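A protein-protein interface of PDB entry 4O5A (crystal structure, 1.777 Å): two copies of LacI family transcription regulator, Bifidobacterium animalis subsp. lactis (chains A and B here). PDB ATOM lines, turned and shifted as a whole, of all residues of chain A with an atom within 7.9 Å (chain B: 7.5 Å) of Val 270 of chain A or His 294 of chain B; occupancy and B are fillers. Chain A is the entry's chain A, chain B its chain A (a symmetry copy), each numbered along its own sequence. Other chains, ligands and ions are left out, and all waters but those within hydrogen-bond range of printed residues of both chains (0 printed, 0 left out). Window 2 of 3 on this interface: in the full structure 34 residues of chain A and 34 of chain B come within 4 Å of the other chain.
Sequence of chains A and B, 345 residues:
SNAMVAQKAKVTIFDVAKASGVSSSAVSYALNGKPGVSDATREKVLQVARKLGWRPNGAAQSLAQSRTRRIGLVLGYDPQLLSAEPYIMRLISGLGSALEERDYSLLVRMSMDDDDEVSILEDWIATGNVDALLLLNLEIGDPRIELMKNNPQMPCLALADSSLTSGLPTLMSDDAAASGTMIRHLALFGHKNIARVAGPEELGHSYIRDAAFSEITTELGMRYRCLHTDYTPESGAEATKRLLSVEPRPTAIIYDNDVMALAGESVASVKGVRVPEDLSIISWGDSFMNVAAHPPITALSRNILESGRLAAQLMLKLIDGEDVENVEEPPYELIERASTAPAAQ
The side-chain hydroxyl (OG) of Ser 266 of chain A is in hydrogen-bond range of the backbone carbonyl oxygen (O) of Ala 292 of chain B (2.6 Å).
OG of Ser 266 of chain A sits close to O of Ala 293 of chain B, 3.5 Å away.
The backbone carbonyl oxygen (O) of Ala 292 of chain B sits close to the backbone carbonyl oxygen (O) of Leu 262 of chain A (3.5 Å).
The backbone carbonyl oxygen (O) of Leu 262 of chain A sits at hydrogen-bond distance from the side-chain hydroxyl (OG) of Ser 266 of chain A, 3.2 Å away.
OG of Ser 269 of chain A is in hydrogen-bond range of O of Glu 265 of chain A (3.2 Å).
The backbone NH of His 294 of chain A is in hydrogen-bond range of the side-chain carboxylate of Glu 265 of chain A.
O of Leu 262 of chain B is in hydrogen-bond range of OG of Ser 266 of chain B, at 3.2 Å.
O of Glu 265 of chain B sits at hydrogen-bond distance from OG of Ser 269 of chain B, at 3.2 Å.
The backbone NH (N) of His 294 of chain B is in hydrogen-bond range of the side-chain carboxylate (OE1) of Glu 265 of chain B (3.3 Å).
CD2 of Leu 262 of chain B touches CD2 of Leu 262 of chain A, at 3.8 Å.
Met 289 of chain B touches Leu 262 of chain A (O to CD2, 3.8 Å).
Ala 292 of chain B touches Ala 263 of chain A.
Ser 266 of chain A touches His 294 of chain B.
His 294 of chain B touches Ser 269 of chain A.
Val 270 of chain A touches His 294 of chain B (CG2 to CE1, 3.6 Å).
Ser 266 of chain B touches His 294 of chain A.
His 294 of chain A touches Ser 269 of chain B.
Val 270 of chain A touches one residue of chain B.
His 294 of chain B touches just these residues of chain A: Ser 266 (3.4 Å), Ser 269 (3.5 Å) and Val 270 (3.6 Å).
No residue of chain A comes within 4 Å of Pro 295 of chain B.
Of the printed residues of chain A, Met 289 of chain B touches Leu 262 (3.8 Å).
Of the printed residues of chain B, Leu 262 of chain A touches Leu 262, Met 289 and Ala 292.
Of the printed residues of chain B, Ser 266 of chain A touches Ala 292 (2.6 Å), Ala 293 (3.3 Å) and His 294 (3.4 Å).
Lys 271 of chain A touches none of the printed residues of chain B.
Gly 264 of chain A touches none of the printed residues of chain B.
The nearest printed residue of chain A that does not touch Met 289 of chain B is Ser 266 of chain A (7.0 Å).
Of the 16 printed residues of chain B, 7 touch a printed residue of chain A.
Hydrophobic or aromatic side chains of chain B within 4 Å of the printed part of chain A: Leu 262, Ala 292 and His 294.
Of the 15 printed residues of chain A, 6 touch a printed residue of chain B.
Among the printed residues, 11 pairs touch across the chains.
Leu 262 of chain B touches its own counterpart, Leu 262 of chain A.
Ser 266 of chain A touches His 294 of chain B, and with the chains exchanged His 294 of chain A touches Ser 266 of chain B.
Ser 269 of chain A touches His 294 of chain B, and with the chains exchanged His 294 of chain A touches Ser 269 of chain B.
Of the 11 pairs that touch across the chains among the printed residues, 5 have their exchanged pair printed and touching as well.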
ATOM      1  N   LYS A 241      19.791  23.878 -14.787  1.00  0.00           N
ATOM      2  CA  LYS A 241      20.515  24.999 -14.194  1.00  0.00           C
ATOM      3  C   LYS A 241      19.794  25.507 -12.951  1.00  0.00           C
ATOM      4  O   LYS A 241      20.413  25.789 -11.919  1.00  0.00           O
ATOM      5  CB  LYS A 241      20.640  26.140 -15.204  1.00  0.00           C
ATOM      6  CG  LYS A 241      21.692  25.918 -16.284  1.00  0.00           C
ATOM      7  CD  LYS A 241      21.829  27.187 -17.132  1.00  0.00           C
ATOM      8  CE  LYS A 241      22.914  27.037 -18.186  1.00  0.00           C
ATOM      9  NZ  LYS A 241      23.305  28.359 -18.768  1.00  0.00           N
ATOM     10  N   LEU A 262      19.904  14.152 -21.468  1.00  0.00           N
ATOM     11  CA  LEU A 262      21.209  14.452 -22.057  1.00  0.00           C
ATOM     12  C   LEU A 262      21.586  15.925 -21.872  1.00  0.00           C
ATOM     13  O   LEU A 262      22.712  16.242 -21.483  1.00  0.00           O
ATOM     14  CB  LEU A 262      21.226  14.074 -23.547  1.00  0.00           C
ATOM     15  CG  LEU A 262      22.539  14.401 -24.258  1.00  0.00           C
ATOM     16  CD1 LEU A 262      23.653  13.560 -23.658  1.00  0.00           C
ATOM     17  CD2 LEU A 262      22.392  14.088 -25.735  1.00  0.00           C
ATOM     18  N   ALA A 263      20.651  16.829 -22.149  1.00  0.00           N
ATOM     19  CA  ALA A 263      20.909  18.268 -22.011  1.00  0.00           C
ATOM     20  C   ALA A 263      21.263  18.607 -20.568  1.00  0.00           C
ATOM     21  O   ALA A 263      22.158  19.417 -20.300  1.00  0.00           O
ATOM     22  CB  ALA A 263      19.684  19.074 -22.474  1.00  0.00           C
ATOM     23  N   GLY A 264      20.557  17.971 -19.640  1.00  0.00           N
ATOM     24  CA  GLY A 264      20.821  18.129 -18.211  1.00  0.00           C
ATOM     25  C   GLY A 264      22.160  17.572 -17.783  1.00  0.00           C
ATOM     26  O   GLY A 264      22.878  18.183 -16.989  1.00  0.00           O
ATOM     27  N   GLU A 265      22.522  16.414 -18.315  1.00  0.00           N
ATOM     28  CA  GLU A 265      23.852  15.861 -18.030  1.00  0.00           C
ATOM     29  C   GLU A 265      24.954  16.806 -18.527  1.00  0.00           C
ATOM     30  O   GLU A 265      25.960  17.013 -17.853  1.00  0.00           O
ATOM     31  CB  GLU A 265      23.997  14.489 -18.685  1.00  0.00           C
ATOM     32  CG  GLU A 265      25.267  13.743 -18.346  1.00  0.00           C
ATOM     33  CD  GLU A 265      25.368  12.455 -19.144  1.00  0.00           C
ATOM     34  OE1 GLU A 265      25.462  12.549 -20.387  1.00  0.00           O
ATOM     35  OE2 GLU A 265      25.337  11.358 -18.545  1.00  0.00           O
ATOM     36  N   SER A 266      24.761  17.382 -19.707  1.00  0.00           N
ATOM     37  CA  SER A 266      25.737  18.326 -20.250  1.00  0.00           C
ATOM     38  C   SER A 266      25.827  19.587 -19.388  1.00  0.00           C
ATOM     39  O   SER A 266      26.922  20.105 -19.151  1.00  0.00           O
ATOM     40  CB  SER A 266      25.415  18.670 -21.711  1.00  0.00           C
ATOM     41  OG  SER A 266      25.443  17.491 -22.509  1.00  0.00           O
ATOM     42  N   VAL A 267      24.685  20.068 -18.906  1.00  0.00           N
ATOM     43  CA  VAL A 267      24.672  21.208 -17.981  1.00  0.00           C
ATOM     44  C   VAL A 267      25.473  20.901 -16.723  1.00  0.00           C
ATOM     45  O   VAL A 267      26.281  21.718 -16.287  1.00  0.00           O
ATOM     46  CB  VAL A 267      23.221  21.622 -17.582  1.00  0.00           C
ATOM     47  CG1 VAL A 267      23.224  22.457 -16.287  1.00  0.00           C
ATOM     48  CG2 VAL A 267      22.574  22.419 -18.712  1.00  0.00           C
ATOM     49  N   ALA A 268      25.241  19.732 -16.141  1.00  0.00           N
ATOM     50  CA  ALA A 268      25.971  19.352 -14.934  1.00  0.00           C
ATOM     51  C   ALA A 268      27.479  19.328 -15.206  1.00  0.00           C
ATOM     52  O   ALA A 268      28.271  19.844 -14.418  1.00  0.00           O
ATOM     53  CB  ALA A 268      25.489  18.009 -14.419  1.00  0.00           C
ATOM     54  N   SER A 269      27.875  18.754 -16.341  1.00  0.00           N
ATOM     55  CA  SER A 269      29.300  18.662 -16.663  1.00  0.00           C
ATOM     56  C   SER A 269      29.928  20.029 -16.802  1.00  0.00           C
ATOM     57  O   SER A 269      31.013  20.261 -16.281  1.00  0.00           O
ATOM     58  CB  SER A 269      29.543  17.843 -17.931  1.00  0.00           C
ATOM     59  OG  SER A 269      29.103  16.506 -17.730  1.00  0.00           O
ATOM     60  N   VAL A 270      29.258  20.935 -17.511  1.00  0.00           N
ATOM     61  CA  VAL A 270      29.798  22.284 -17.693  1.00  0.00           C
ATOM     62  C   VAL A 270      29.935  22.961 -16.332  1.00  0.00           C
ATOM     63  O   VAL A 270      30.881  23.712 -16.079  1.00  0.00           O
ATOM     64  CB  VAL A 270      28.880  23.110 -18.624  1.00  0.00           C
ATOM     65  CG1 VAL A 270      29.246  24.590 -18.599  1.00  0.00           C
ATOM     66  CG2 VAL A 270      28.930  22.557 -20.038  1.00  0.00           C
ATOM     67  N   LYS A 271      29.009  22.647 -15.435  1.00  0.00           N
ATOM     68  CA  LYS A 271      28.970  23.268 -14.107  1.00  0.00           C
ATOM     69  C   LYS A 271      29.983  22.636 -13.136  1.00  0.00           C
ATOM     70  O   LYS A 271      30.257  23.188 -12.075  1.00  0.00           O
ATOM     71  CB  LYS A 271      27.546  23.155 -13.545  1.00  0.00           C
ATOM     72  CG  LYS A 271      27.154  24.153 -12.460  1.00  0.00           C
ATOM     73  CD  LYS A 271      25.630  24.076 -12.218  1.00  0.00           C
ATOM     74  CE  LYS A 271      25.172  24.929 -11.040  1.00  0.00           C
ATOM     75  NZ  LYS A 271      25.486  26.369 -11.220  1.00  0.00           N
ATOM     76  N   GLY A 272      30.545  21.486 -13.505  1.00  0.00           N
ATOM     77  CA  GLY A 272      31.493  20.802 -12.639  1.00  0.00           C
ATOM     78  C   GLY A 272      30.788  19.887 -11.645  1.00  0.00           C
ATOM     79  O   GLY A 272      31.394  19.389 -10.690  1.00  0.00           O
ATOM     80  N   VAL A 273      29.502  19.676 -11.859  1.00  0.00           N
ATOM     81  CA  VAL A 273      28.747  18.717 -11.068  1.00  0.00           C
ATOM     82  C   VAL A 273      28.889  17.345 -11.721  1.00  0.00           C
ATOM     83  O   VAL A 273      28.344  17.103 -12.795  1.00  0.00           O
ATOM     84  CB  VAL A 273      27.279  19.137 -10.998  1.00  0.00           C
ATOM     85  CG1 VAL A 273      26.439  18.087 -10.276  1.00  0.00           C
ATOM     86  CG2 VAL A 273      27.172  20.496 -10.304  1.00  0.00           C
ATOM     87  N   ARG A 274      29.638  16.456 -11.073  1.00  0.00           N
ATOM     88  CA  ARG A 274      29.934  15.131 -11.629  1.00  0.00           C
ATOM     89  C   ARG A 274      28.716  14.219 -11.687  1.00  0.00           C
ATOM     90  O   ARG A 274      27.959  14.119 -10.723  1.00  0.00           O
ATOM     91  CB  ARG A 274      31.025  14.444 -10.804  1.00  0.00           C
ATOM     92  CG  ARG A 274      32.367  15.169 -10.841  1.00  0.00           C
ATOM     93  CD  ARG A 274      33.330  14.523  -9.873  1.00  0.00           C
ATOM     94  NE  ARG A 274      32.850  14.631  -8.495  1.00  0.00           N
ATOM     95  CZ  ARG A 274      33.341  13.937  -7.472  1.00  0.00           C
ATOM     96  NH1 ARG A 274      34.323  13.067  -7.666  1.00  0.00           N
ATOM     97  NH2 ARG A 274      32.841  14.106  -6.254  1.00  0.00           N
ATOM     98  N   HIS A 294      27.562  10.607 -21.960  1.00  0.00           N
ATOM     99  CA  HIS A 294      28.800  10.639 -21.160  1.00  0.00           C
ATOM    100  C   HIS A 294      28.539  11.083 -19.720  1.00  0.00           C
ATOM    101  O   HIS A 294      28.577  12.274 -19.424  1.00  0.00           O
ATOM    102  CB  HIS A 294      29.797  11.604 -21.817  1.00  0.00           C
ATOM    103  CG  HIS A 294      31.097  11.707 -21.092  1.00  0.00           C
ATOM    104  ND1 HIS A 294      31.849  10.602 -20.750  1.00  0.00           N
ATOM    105  CD2 HIS A 294      31.800  12.784 -20.657  1.00  0.00           C
ATOM    106  CE1 HIS A 294      32.946  10.992 -20.126  1.00  0.00           C
ATOM    107  NE2 HIS A 294      32.938  12.316 -20.060  1.00  0.00           N
ATOM    108  N   LEU B 262      27.584  11.495 -31.227  1.00  0.00           N
ATOM    109  CA  LEU B 262      27.517  11.575 -29.768  1.00  0.00           C
ATOM    110  C   LEU B 262      28.347  10.472 -29.103  1.00  0.00           C
ATOM    111  O   LEU B 262      29.105  10.735 -28.167  1.00  0.00           O
ATOM    112  CB  LEU B 262      26.056  11.509 -29.293  1.00  0.00           C
ATOM    113  CG  LEU B 262      25.892  11.535 -27.773  1.00  0.00           C
ATOM    114  CD1 LEU B 262      26.386  12.871 -27.243  1.00  0.00           C
ATOM    115  CD2 LEU B 262      24.426  11.353 -27.431  1.00  0.00           C
ATOM    116  N   GLU B 265      31.927  11.371 -29.483  1.00  0.00           N
ATOM    117  CA  GLU B 265      32.310  12.450 -28.564  1.00  0.00           C
ATOM    118  C   GLU B 265      32.520  11.908 -27.144  1.00  0.00           C
ATOM    119  O   GLU B 265      33.457  12.299 -26.451  1.00  0.00           O
ATOM    120  CB  GLU B 265      31.236  13.537 -28.562  1.00  0.00           C
ATOM    121  CG  GLU B 265      31.577  14.778 -27.768  1.00  0.00           C
ATOM    122  CD  GLU B 265      30.398  15.735 -27.728  1.00  0.00           C
ATOM    123  OE1 GLU B 265      29.359  15.350 -27.151  1.00  0.00           O
ATOM    124  OE2 GLU B 265      30.496  16.853 -28.280  1.00  0.00           O
ATOM    125  N   SER B 266      31.647  11.005 -26.713  1.00  0.00           N
ATOM    126  CA  SER B 266      31.784  10.403 -25.387  1.00  0.00           C
ATOM    127  C   SER B 266      33.058   9.562 -25.290  1.00  0.00           C
ATOM    128  O   SER B 266      33.752   9.592 -24.269  1.00  0.00           O
ATOM    129  CB  SER B 266      30.541   9.578 -25.028  1.00  0.00           C
ATOM    130  OG  SER B 266      29.386  10.411 -25.023  1.00  0.00           O
ATOM    131  N   SER B 269      35.963  11.916 -24.853  1.00  0.00           N
ATOM    132  CA  SER B 269      36.011  12.460 -23.495  1.00  0.00           C
ATOM    133  C   SER B 269      36.579  11.460 -22.515  1.00  0.00           C
ATOM    134  O   SER B 269      37.410  11.818 -21.688  1.00  0.00           O
ATOM    135  CB  SER B 269      34.635  12.932 -23.024  1.00  0.00           C
ATOM    136  OG  SER B 269      34.182  13.993 -23.853  1.00  0.00           O
ATOM    137  N   VAL B 275      37.234  17.716 -27.010  1.00  0.00           N
ATOM    138  CA  VAL B 275      36.449  18.204 -28.146  1.00  0.00           C
ATOM    139  C   VAL B 275      36.030  19.632 -27.793  1.00  0.00           C
ATOM    140  O   VAL B 275      35.352  19.838 -26.794  1.00  0.00           O
ATOM    141  CB  VAL B 275      35.204  17.326 -28.373  1.00  0.00           C
ATOM    142  CG1 VAL B 275      34.309  17.912 -29.480  1.00  0.00           C
ATOM    143  CG2 VAL B 275      35.622  15.898 -28.729  1.00  0.00           C
ATOM    144  N   MET B 289      19.510  16.067 -30.299  1.00  0.00           N
ATOM    145  CA  MET B 289      20.603  15.377 -29.634  1.00  0.00           C
ATOM    146  C   MET B 289      21.905  16.171 -29.755  1.00  0.00           C
ATOM    147  O   MET B 289      22.689  16.261 -28.809  1.00  0.00           O
ATOM    148  CB  MET B 289      20.769  14.009 -30.287  1.00  0.00           C
ATOM    149  CG  MET B 289      21.734  13.083 -29.629  1.00  0.00           C
ATOM    150  SD  MET B 289      21.899  11.505 -30.771  1.00  0.00           S
ATOM    151  CE  MET B 289      20.029  11.194 -31.183  1.00  0.00           C
ATOM    152  N   ASN B 290      22.134  16.741 -30.927  1.00  0.00           N
ATOM    153  CA  ASN B 290      23.332  17.536 -31.167  1.00  0.00           C
ATOM    154  C   ASN B 290      23.372  18.812 -30.332  1.00  0.00           C
ATOM    155  O   ASN B 290      24.454  19.265 -29.942  1.00  0.00           O
ATOM    156  CB  ASN B 290      23.481  17.852 -32.661  1.00  0.00           C
ATOM    157  CG  ASN B 290      23.874  16.630 -33.468  1.00  0.00           C
ATOM    158  OD1 ASN B 290      24.549  15.718 -32.955  1.00  0.00           O
ATOM    159  ND2 ASN B 290      23.438  16.585 -34.724  1.00  0.00           N
ATOM    160  N   VAL B 291      22.201  19.381 -30.057  1.00  0.00           N
ATOM    161  CA  VAL B 291      22.092  20.607 -29.278  1.00  0.00           C
ATOM    162  C   VAL B 291      22.373  20.312 -27.807  1.00  0.00           C
ATOM    163  O   VAL B 291      22.877  21.160 -27.070  1.00  0.00           O
ATOM    164  CB  VAL B 291      20.696  21.216 -29.456  1.00  0.00           C
ATOM    165  CG1 VAL B 291      20.467  22.389 -28.521  1.00  0.00           C
ATOM    166  CG2 VAL B 291      20.523  21.666 -30.925  1.00  0.00           C
ATOM    167  N   ALA B 292      22.048  19.092 -27.392  1.00  0.00           N
ATOM    168  CA  ALA B 292      22.102  18.700 -25.985  1.00  0.00           C
ATOM    169  C   ALA B 292      23.441  18.120 -25.572  1.00  0.00           C
ATOM    170  O   ALA B 292      23.651  17.851 -24.392  1.00  0.00           O
ATOM    171  CB  ALA B 292      20.992  17.670 -25.664  1.00  0.00           C
ATOM    172  N   ALA B 293      24.324  17.903 -26.541  1.00  0.00           N
ATOM    173  CA  ALA B 293      25.595  17.196 -26.304  1.00  0.00           C
ATOM    174  C   ALA B 293      26.623  18.057 -25.565  1.00  0.00           C
ATOM    175  O   ALA B 293      26.403  19.248 -25.331  1.00  0.00           O
ATOM    176  CB  ALA B 293      26.183  16.724 -27.628  1.00  0.00           C
ATOM    177  N   HIS B 294      27.758  17.447 -25.226  1.00  0.00           N
ATOM    178  CA  HIS B 294      28.799  18.114 -24.423  1.00  0.00           C
ATOM    179  C   HIS B 294      30.178  18.014 -25.076  1.00  0.00           C
ATOM    180  O   HIS B 294      30.910  17.059 -24.831  1.00  0.00           O
ATOM    181  CB  HIS B 294      28.848  17.470 -23.030  1.00  0.00           C
ATOM    182  CG  HIS B 294      29.865  18.079 -22.125  1.00  0.00           C
ATOM    183  ND1 HIS B 294      29.935  19.437 -21.889  1.00  0.00           N
ATOM    184  CD2 HIS B 294      30.849  17.520 -21.374  1.00  0.00           C
ATOM    185  CE1 HIS B 294      30.923  19.687 -21.047  1.00  0.00           C
ATOM    186  NE2 HIS B 294      31.490  18.535 -20.719  1.00  0.00           N
ATOM    187  N   PRO B 295      30.556  18.995 -25.908  1.00  0.00           N
ATOM    188  CA  PRO B 295      29.836  20.216 -26.281  1.00  0.00           C
ATOM    189  C   PRO B 295      28.833  19.962 -27.405  1.00  0.00           C
ATOM    190  O   PRO B 295      28.852  18.894 -28.038  1.00  0.00           O
ATOM    191  CB  PRO B 295      30.963  21.119 -26.782  1.00  0.00           C
ATOM    192  CG  PRO B 295      31.931  20.154 -27.414  1.00  0.00           C
ATOM    193  CD  PRO B 295      31.921  18.978 -26.476  1.00  0.00           C
ATOM    194  N   PRO B 296      27.952  20.931 -27.649  1.00  0.00           N
ATOM    195  CA  PRO B 296      27.010  20.776 -28.765  1.00  0.00           C
ATOM    196  C   PRO B 296      27.729  20.523 -30.099  1.00  0.00           C
ATOM    197  O   PRO B 296      28.803  21.073 -30.381  1.00  0.00           O
ATOM    198  CB  PRO B 296      26.268  22.110 -28.777  1.00  0.00           C
ATOM    199  CG  PRO B 296      26.319  22.563 -27.341  1.00  0.00           C
ATOM    200  CD  PRO B 296      27.700  22.154 -26.873  1.00  0.00           C
ATOM    201  N   ILE B 297      27.118  19.670 -30.915  1.00  0.00           N
ATOM    202  CA  ILE B 297      27.782  19.095 -32.078  1.00  0.00           C
ATOM    203  C   ILE B 297      27.372  19.786 -33.388  1.00  0.00           C
ATOM    204  O   ILE B 297      26.181  19.878 -33.725  1.00  0.00           O
ATOM    205  CB  ILE B 297      27.506  17.575 -32.153  1.00  0.00           C
ATOM    206  CG1 ILE B 297      28.059  16.864 -30.895  1.00  0.00           C
ATOM    207  CG2 ILE B 297      28.122  16.968 -33.414  1.00  0.00           C
ATOM    208  CD1 ILE B 297      27.753  15.364 -30.848  1.00  0.00           C
ATOM    209  N   ALA B 338      29.760  24.106 -31.084  1.00  0.00           N
ATOM    210  CA  ALA B 338      31.004  24.149 -30.334  1.00  0.00           C
ATOM    211  C   ALA B 338      31.983  23.027 -30.653  1.00  0.00           C
ATOM    212  O   ALA B 338      33.165  23.130 -30.312  1.00  0.00           O
ATOM    213  CB  ALA B 338      30.705  24.183 -28.841  1.00  0.00           C
ATOM    214  N   SER B 339      31.521  21.970 -31.316  1.00  0.00           N
ATOM    215  CA  SER B 339      32.371  20.789 -31.524  1.00  0.00           C
ATOM    216  C   SER B 339      33.363  20.885 -32.696  1.00  0.00           C
ATOM    217  O   SER B 339      34.107  19.933 -32.939  1.00  0.00           O
ATOM    218  CB  SER B 339      31.513  19.520 -31.680  1.00  0.00           C
ATOM    219  OG  SER B 339      30.880  19.520 -32.958  1.00  0.00           O
